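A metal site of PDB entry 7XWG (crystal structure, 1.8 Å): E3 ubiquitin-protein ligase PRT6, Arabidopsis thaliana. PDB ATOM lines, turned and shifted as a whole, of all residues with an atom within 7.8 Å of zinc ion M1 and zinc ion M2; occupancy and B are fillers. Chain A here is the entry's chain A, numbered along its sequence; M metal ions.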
ATOM      1  N   GLY A   7      18.045 -28.016  -0.338  1.00  0.00           N
ATOM      2  CA  GLY A   7      18.260 -29.410   0.006  1.00  0.00           C
ATOM      3  C   GLY A   7      18.031 -29.699   1.477  1.00  0.00           C
ATOM      4  O   GLY A   7      18.387 -28.895   2.351  1.00  0.00           O
ATOM      5  N   VAL A   8      17.401 -30.819   1.762  1.00  0.00           N
ATOM      6  CA  VAL A   8      17.117 -31.318   3.108  1.00  0.00           C
ATOM      7  C   VAL A   8      18.294 -32.160   3.628  1.00  0.00           C
ATOM      8  O   VAL A   8      18.876 -32.962   2.880  1.00  0.00           O
ATOM      9  CB  VAL A   8      15.808 -32.118   3.080  1.00  0.00           C
ATOM     10  CG1 VAL A   8      15.422 -32.565   4.448  1.00  0.00           C
ATOM     11  CG2 VAL A   8      14.728 -31.261   2.433  1.00  0.00           C
ATOM     12  N   CYS A   9      18.651 -32.006   4.909  1.00  0.00           N
ATOM     13  CA  CYS A   9      19.606 -32.889   5.557  1.00  0.00           C
ATOM     14  C   CYS A   9      19.090 -34.309   5.711  1.00  0.00           C
ATOM     15  O   CYS A   9      17.959 -34.520   6.186  1.00  0.00           O
ATOM     16  CB  CYS A   9      19.957 -32.263   6.938  1.00  0.00           C
ATOM     17  SG  CYS A   9      20.994 -33.308   8.174  1.00  0.00           S
ATOM     18  N   GLY A  10      19.928 -35.281   5.358  1.00  0.00           N
ATOM     19  CA  GLY A  10      19.587 -36.678   5.475  1.00  0.00           C
ATOM     20  C   GLY A  10      20.102 -37.356   6.736  1.00  0.00           C
ATOM     21  O   GLY A  10      20.096 -38.598   6.816  1.00  0.00           O
ATOM     22  N   SER A  11      20.542 -36.584   7.718  1.00  0.00           N
ATOM     23  CA  SER A  11      21.117 -37.186   8.907  1.00  0.00           C
ATOM     24  C   SER A  11      20.032 -37.831   9.772  1.00  0.00           C
ATOM     25  O   SER A  11      18.865 -37.479   9.742  1.00  0.00           O
ATOM     26  CB  SER A  11      21.864 -36.143   9.724  1.00  0.00           C
ATOM     27  OG  SER A  11      23.193 -36.064   9.299  1.00  0.00           O
ATOM     28  N   VAL A  12      20.485 -38.724  10.618  1.00  0.00           N
ATOM     29  CA  VAL A  12      19.600 -39.631  11.314  1.00  0.00           C
ATOM     30  C   VAL A  12      20.185 -39.845  12.691  1.00  0.00           C
ATOM     31  O   VAL A  12      21.391 -39.686  12.886  1.00  0.00           O
ATOM     32  CB  VAL A  12      19.518 -40.923  10.468  1.00  0.00           C
ATOM     33  CG1 VAL A  12      19.264 -42.006  11.286  1.00  0.00           C
ATOM     34  CG2 VAL A  12      18.487 -40.779   9.367  1.00  0.00           C
ATOM     35  N   TRP A  13      19.340 -40.161  13.661  1.00  0.00           N
ATOM     36  CA  TRP A  13      19.883 -40.606  14.940  1.00  0.00           C
ATOM     37  C   TRP A  13      19.059 -41.761  15.502  1.00  0.00           C
ATOM     38  O   TRP A  13      17.917 -42.004  15.093  1.00  0.00           O
ATOM     39  CB  TRP A  13      19.974 -39.470  15.965  1.00  0.00           C
ATOM     40  CG  TRP A  13      18.696 -38.804  16.258  1.00  0.00           C
ATOM     41  CD1 TRP A  13      17.801 -39.106  17.251  1.00  0.00           C
ATOM     42  CD2 TRP A  13      18.139 -37.696  15.546  1.00  0.00           C
ATOM     43  NE1 TRP A  13      16.706 -38.245  17.184  1.00  0.00           N
ATOM     44  CE2 TRP A  13      16.896 -37.380  16.131  1.00  0.00           C
ATOM     45  CE3 TRP A  13      18.558 -36.960  14.437  1.00  0.00           C
ATOM     46  CZ2 TRP A  13      16.084 -36.328  15.665  1.00  0.00           C
ATOM     47  CZ3 TRP A  13      17.755 -35.913  13.975  1.00  0.00           C
ATOM     48  CH2 TRP A  13      16.525 -35.618  14.588  1.00  0.00           C
ATOM     49  N   ALA A  32      12.591 -31.905  14.918  1.00  0.00           N
ATOM     50  CA  ALA A  32      13.894 -31.915  15.568  1.00  0.00           C
ATOM     51  C   ALA A  32      14.967 -31.894  14.495  1.00  0.00           C
ATOM     52  O   ALA A  32      14.733 -32.295  13.346  1.00  0.00           O
ATOM     53  CB  ALA A  32      14.017 -33.128  16.479  1.00  0.00           C
ATOM     54  N   ILE A  33      16.153 -31.422  14.875  1.00  0.00           N
ATOM     55  CA  ILE A  33      17.311 -31.382  13.979  1.00  0.00           C
ATOM     56  C   ILE A  33      18.529 -31.978  14.680  1.00  0.00           C
ATOM     57  O   ILE A  33      18.596 -32.006  15.910  1.00  0.00           O
ATOM     58  CB  ILE A  33      17.619 -29.939  13.527  1.00  0.00           C
ATOM     59  CG1 ILE A  33      17.915 -29.052  14.723  1.00  0.00           C
ATOM     60  CG2 ILE A  33      16.413 -29.370  12.790  1.00  0.00           C
ATOM     61  CD1 ILE A  33      18.399 -27.640  14.335  1.00  0.00           C
ATOM     62  N   CYS A  34      19.477 -32.481  13.872  1.00  0.00           N
ATOM     63  CA  CYS A  34      20.695 -33.085  14.414  1.00  0.00           C
ATOM     64  C   CYS A  34      21.591 -32.037  15.049  1.00  0.00           C
ATOM     65  O   CYS A  34      21.449 -30.830  14.835  1.00  0.00           O
ATOM     66  CB  CYS A  34      21.473 -33.836  13.315  1.00  0.00           C
ATOM     67  SG  CYS A  34      22.151 -32.754  11.996  1.00  0.00           S
ATOM     68  N   VAL A  35      22.519 -32.500  15.869  1.00  0.00           N
ATOM     69  CA  VAL A  35      23.393 -31.572  16.572  1.00  0.00           C
ATOM     70  C   VAL A  35      24.193 -30.700  15.616  1.00  0.00           C
ATOM     71  O   VAL A  35      24.271 -29.489  15.851  1.00  0.00           O
ATOM     72  CB  VAL A  35      24.272 -32.331  17.576  1.00  0.00           C
ATOM     73  CG1 VAL A  35      25.341 -31.405  18.156  1.00  0.00           C
ATOM     74  CG2 VAL A  35      23.374 -32.910  18.639  1.00  0.00           C
ATOM     75  N   PRO A  36      24.851 -31.233  14.580  1.00  0.00           N
ATOM     76  CA  PRO A  36      25.612 -30.345  13.683  1.00  0.00           C
ATOM     77  C   PRO A  36      24.728 -29.283  13.020  1.00  0.00           C
ATOM     78  O   PRO A  36      25.131 -28.124  12.896  1.00  0.00           O
ATOM     79  CB  PRO A  36      26.228 -31.311  12.655  1.00  0.00           C
ATOM     80  CG  PRO A  36      26.307 -32.634  13.402  1.00  0.00           C
ATOM     81  CD  PRO A  36      25.096 -32.658  14.299  1.00  0.00           C
ATOM     82  N   CYS A  37      23.523 -29.663  12.603  1.00  0.00           N
ATOM     83  CA  CYS A  37      22.621 -28.678  12.027  1.00  0.00           C
ATOM     84  C   CYS A  37      22.273 -27.602  13.031  1.00  0.00           C
ATOM     85  O   CYS A  37      22.260 -26.407  12.693  1.00  0.00           O
ATOM     86  CB  CYS A  37      21.376 -29.389  11.491  1.00  0.00           C
ATOM     87  SG  CYS A  37      21.710 -30.135   9.905  1.00  0.00           S
ATOM     88  N   PHE A  38      21.988 -27.979  14.279  1.00  0.00           N
ATOM     89  CA  PHE A  38      21.753 -26.978  15.320  1.00  0.00           C
ATOM     90  C   PHE A  38      22.979 -26.091  15.523  1.00  0.00           C
ATOM     91  O   PHE A  38      22.861 -24.865  15.602  1.00  0.00           O
ATOM     92  CB  PHE A  38      21.348 -27.658  16.619  1.00  0.00           C
ATOM     93  CG  PHE A  38      21.047 -26.696  17.737  1.00  0.00           C
ATOM     94  CD1 PHE A  38      19.758 -26.221  17.938  1.00  0.00           C
ATOM     95  CD2 PHE A  38      22.058 -26.250  18.569  1.00  0.00           C
ATOM     96  CE1 PHE A  38      19.491 -25.347  18.938  1.00  0.00           C
ATOM     97  CE2 PHE A  38      21.789 -25.353  19.577  1.00  0.00           C
ATOM     98  CZ  PHE A  38      20.501 -24.910  19.761  1.00  0.00           C
ATOM     99  N   ASN A  40      25.302 -25.289  13.490  1.00  0.00           N
ATOM    100  CA  ASN A  40      25.580 -24.451  12.332  1.00  0.00           C
ATOM    101  C   ASN A  40      24.444 -23.490  12.027  1.00  0.00           C
ATOM    102  O   ASN A  40      24.435 -22.882  10.951  1.00  0.00           O
ATOM    103  CB  ASN A  40      25.859 -25.312  11.111  1.00  0.00           C
ATOM    104  CG  ASN A  40      27.206 -25.989  11.174  1.00  0.00           C
ATOM    105  OD1 ASN A  40      28.190 -25.391  11.598  1.00  0.00           O
ATOM    106  ND2 ASN A  40      27.256 -27.251  10.733  1.00  0.00           N
ATOM    107  N   GLY A  41      23.485 -23.353  12.922  1.00  0.00           N
ATOM    108  CA  GLY A  41      22.442 -22.365  12.786  1.00  0.00           C
ATOM    109  C   GLY A  41      22.524 -21.394  13.931  1.00  0.00           C
ATOM    110  O   GLY A  41      23.446 -21.466  14.741  1.00  0.00           O
ATOM    111  N   CYS A  57      14.799 -38.528  12.081  1.00  0.00           N
ATOM    112  CA  CYS A  57      15.415 -37.937  10.918  1.00  0.00           C
ATOM    113  C   CYS A  57      15.400 -36.421  11.090  1.00  0.00           C
ATOM    114  O   CYS A  57      14.398 -35.847  11.532  1.00  0.00           O
ATOM    115  CB  CYS A  57      14.636 -38.310   9.649  1.00  0.00           C
ATOM    116  SG  CYS A  57      14.697 -40.066   9.209  1.00  0.00           S
ATOM    117  N   CYS A  58      16.495 -35.799  10.677  1.00  0.00           N
ATOM    118  CA  CYS A  58      16.688 -34.370  10.846  1.00  0.00           C
ATOM    119  C   CYS A  58      15.772 -33.609   9.904  1.00  0.00           C
ATOM    120  O   CYS A  58      15.654 -33.955   8.726  1.00  0.00           O
ATOM    121  CB  CYS A  58      18.150 -34.002  10.588  1.00  0.00           C
ATOM    122  SG  CYS A  58      18.579 -32.245  10.753  1.00  0.00           S
ATOM    123  N   ASP A  59      15.081 -32.604  10.422  1.00  0.00           N
ATOM    124  CA  ASP A  59      14.169 -31.776   9.624  1.00  0.00           C
ATOM    125  C   ASP A  59      14.823 -30.496   9.054  1.00  0.00           C
ATOM    126  O   ASP A  59      14.111 -29.668   8.454  1.00  0.00           O
ATOM    127  CB  ASP A  59      12.979 -31.422  10.490  1.00  0.00           C
ATOM    128  CG  ASP A  59      12.194 -32.651  10.882  1.00  0.00           C
ATOM    129  OD1 ASP A  59      11.932 -33.470   9.999  1.00  0.00           O
ATOM    130  OD2 ASP A  59      11.878 -32.814  12.086  1.00  0.00           O
ATOM    131  N   CYS A  60      16.142 -30.345   9.173  1.00  0.00           N
ATOM    132  CA  CYS A  60      16.814 -29.129   8.711  1.00  0.00           C
ATOM    133  C   CYS A  60      16.683 -29.031   7.196  1.00  0.00           C
ATOM    134  O   CYS A  60      17.016 -29.976   6.472  1.00  0.00           O
ATOM    135  CB  CYS A  60      18.290 -29.133   9.124  1.00  0.00           C
ATOM    136  SG  CYS A  60      19.187 -27.549   8.800  1.00  0.00           S
ATOM    137  N   GLY A  61      16.189 -27.875   6.725  1.00  0.00           N
ATOM    138  CA  GLY A  61      15.964 -27.634   5.312  1.00  0.00           C
ATOM    139  C   GLY A  61      14.595 -28.043   4.808  1.00  0.00           C
ATOM    140  O   GLY A  61      14.308 -27.834   3.622  1.00  0.00           O
ATOM    141  N   TRP A  66      10.264 -27.185   9.609  1.00  0.00           N
ATOM    142  CA  TRP A  66      11.191 -26.269  10.258  1.00  0.00           C
ATOM    143  C   TRP A  66      11.126 -24.945   9.537  1.00  0.00           C
ATOM    144  O   TRP A  66      11.112 -24.924   8.317  1.00  0.00           O
ATOM    145  CB  TRP A  66      12.608 -26.788  10.159  1.00  0.00           C
ATOM    146  CG  TRP A  66      13.522 -26.426  11.263  1.00  0.00           C
ATOM    147  CD1 TRP A  66      14.537 -25.542  11.201  1.00  0.00           C
ATOM    148  CD2 TRP A  66      13.545 -26.974  12.594  1.00  0.00           C
ATOM    149  NE1 TRP A  66      15.190 -25.482  12.404  1.00  0.00           N
ATOM    150  CE2 TRP A  66      14.604 -26.358  13.277  1.00  0.00           C
ATOM    151  CE3 TRP A  66      12.763 -27.911  13.266  1.00  0.00           C
ATOM    152  CZ2 TRP A  66      14.918 -26.652  14.609  1.00  0.00           C
ATOM    153  CZ3 TRP A  66      13.069 -28.212  14.607  1.00  0.00           C
ATOM    154  CH2 TRP A  66      14.148 -27.582  15.263  1.00  0.00           C
ATOM    155  N   GLY A  70      15.497 -21.040  10.776  1.00  0.00           N
ATOM    156  CA  GLY A  70      16.165 -22.023  11.599  1.00  0.00           C
ATOM    157  C   GLY A  70      16.998 -23.027  10.854  1.00  0.00           C
ATOM    158  O   GLY A  70      17.602 -23.914  11.486  1.00  0.00           O
ATOM    159  N   PHE A  71      17.088 -22.915   9.533  1.00  0.00           N
ATOM    160  CA  PHE A  71      17.969 -23.772   8.758  1.00  0.00           C
ATOM    161  C   PHE A  71      19.420 -23.483   9.100  1.00  0.00           C
ATOM    162  O   PHE A  71      19.800 -22.332   9.352  1.00  0.00           O
ATOM    163  CB  PHE A  71      17.762 -23.533   7.266  1.00  0.00           C
ATOM    164  CG  PHE A  71      16.420 -23.967   6.753  1.00  0.00           C
ATOM    165  CD1 PHE A  71      16.048 -23.646   5.450  1.00  0.00           C
ATOM    166  CD2 PHE A  71      15.545 -24.683   7.540  1.00  0.00           C
ATOM    167  CE1 PHE A  71      14.815 -24.036   4.939  1.00  0.00           C
ATOM    168  CE2 PHE A  71      14.314 -25.109   7.033  1.00  0.00           C
ATOM    169  CZ  PHE A  71      13.952 -24.770   5.732  1.00  0.00           C
ATOM    170  N   CYS A  72      20.246 -24.527   9.123  1.00  0.00           N
ATOM    171  CA  CYS A  72      21.690 -24.364   9.252  1.00  0.00           C
ATOM    172  C   CYS A  72      22.253 -23.748   7.982  1.00  0.00           C
ATOM    173  O   CYS A  72      21.572 -23.626   6.953  1.00  0.00           O
ATOM    174  CB  CYS A  72      22.360 -25.705   9.601  1.00  0.00           C
ATOM    175  SG  CYS A  72      22.838 -26.720   8.275  1.00  0.00           S
ATOM    176  N   SER A  73      23.507 -23.331   8.062  1.00  0.00           N
ATOM    177  CA  SER A  73      24.199 -22.695   6.952  1.00  0.00           C
ATOM    178  C   SER A  73      24.411 -23.614   5.757  1.00  0.00           C
ATOM    179  O   SER A  73      24.794 -23.124   4.692  1.00  0.00           O
ATOM    180  CB  SER A  73      25.536 -22.132   7.451  1.00  0.00           C
ATOM    181  OG  SER A  73      26.457 -23.163   7.793  1.00  0.00           O
ATOM    182  N   ASN A  74      24.162 -24.912   5.875  1.00  0.00           N
ATOM    183  CA  ASN A  74      24.443 -25.843   4.790  1.00  0.00           C
ATOM    184  C   ASN A  74      23.203 -26.408   4.113  1.00  0.00           C
ATOM    185  O   ASN A  74      23.337 -27.193   3.174  1.00  0.00           O
ATOM    186  CB  ASN A  74      25.312 -27.007   5.287  1.00  0.00           C
ATOM    187  CG  ASN A  74      26.662 -26.557   5.833  1.00  0.00           C
ATOM    188  OD1 ASN A  74      27.320 -25.687   5.253  1.00  0.00           O
ATOM    189  ND2 ASN A  74      27.069 -27.143   6.951  1.00  0.00           N
ATOM    190  N   HIS A  75      21.997 -26.055   4.569  1.00  0.00           N
ATOM    191  CA  HIS A  75      20.747 -26.567   3.990  1.00  0.00           C
ATOM    192  C   HIS A  75      19.806 -25.402   3.669  1.00  0.00           C
ATOM    193  O   HIS A  75      18.860 -25.146   4.429  1.00  0.00           O
ATOM    194  CB  HIS A  75      20.081 -27.633   4.917  1.00  0.00           C
ATOM    195  CG  HIS A  75      20.990 -28.769   5.234  1.00  0.00           C
ATOM    196  ND1 HIS A  75      21.492 -28.975   6.496  1.00  0.00           N
ATOM    197  CD2 HIS A  75      21.519 -29.733   4.452  1.00  0.00           C
ATOM    198  CE1 HIS A  75      22.336 -30.001   6.470  1.00  0.00           C
ATOM    199  NE2 HIS A  75      22.336 -30.498   5.243  1.00  0.00           N
ATOM    200  N   LYS A  76      20.028 -24.762   2.522  1.00  0.00           N
ATOM    201  CA  LYS A  76      19.303 -23.563   2.050  1.00  0.00           C
ATOM    202  C   LYS A  76      19.872 -22.271   2.663  1.00  0.00           C
ATOM    203  O   LYS A  76      20.510 -22.271   3.728  1.00  0.00           O
ATOM    204  CB  LYS A  76      17.801 -23.655   2.373  1.00  0.00           C
ATOM    205  CG  LYS A  76      16.897 -24.239   1.294  1.00  0.00           C
ATOM    206  CD  LYS A  76      16.612 -25.735   1.558  1.00  0.00           C
ATOM    207  CE  LYS A  76      15.463 -26.265   0.707  1.00  0.00           C
ATOM    208  NZ  LYS A  76      15.823 -26.332  -0.746  1.00  0.00           N
HETATM  209 ZN    ZN M   1      21.158 -28.322   8.368  1.00  0.00          ZN
HETATM  210 ZN    ZN M   2      20.778 -32.234  10.226  1.00  0.00          ZN
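The backbone NH (N) of Cys 60 sits close to the side-chain sulfur (SG) of Cys 58, 3.5 Å away. The backbone NH (N) of Cys 9 sits at hydrogen-bond distance from the backbone carbonyl oxygen (O) of Cys 60 (3.0 Å). The backbone carbonyl oxygen (O) of Ser 11 is in hydrogen-bond range of the backbone NH (N) of Cys 58 (3.1 Å). The side-chain sulfur (SG) of Cys 72 lies close to the backbone NH (N) of Asn 74 (3.3 Å). N of Ser 11 sits close to SG of Cys 9.
Within 4 Å of zinc ion M1: Cys 37, Cys 60, Cys 72 and His 75. Along chain A the residues within 4 Å of zinc ion M1 span positions 37 to 75.
Within 4 Å of zinc ion M2: Cys 9, Cys 34, Cys 37 and Cys 58. The nearest printed residue that does not touch zinc ion M2 is Ser 11 (4.1 Å).
Zinc ion M1 is bound by ND1 of His 75 (2.0 Å), SG of Cys 60 (2.2 Å), SG of Cys 72 (2.3 Å) and SG of Cys 37 (2.4 Å). Zinc ion M1 has four donor atoms within binding distance.
Zinc ion M2 is bound by the side-chain sulfur (SG) of Cys 58 (2.3 Å), the side-chain sulfur (SG) of Cys 34 (2.3 Å), the side-chain sulfur (SG) of Cys 37 (2.3 Å) and the side-chain sulfur (SG) of Cys 9 (2.3 Å). Zinc ion M2 has four donor atoms within binding distance.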
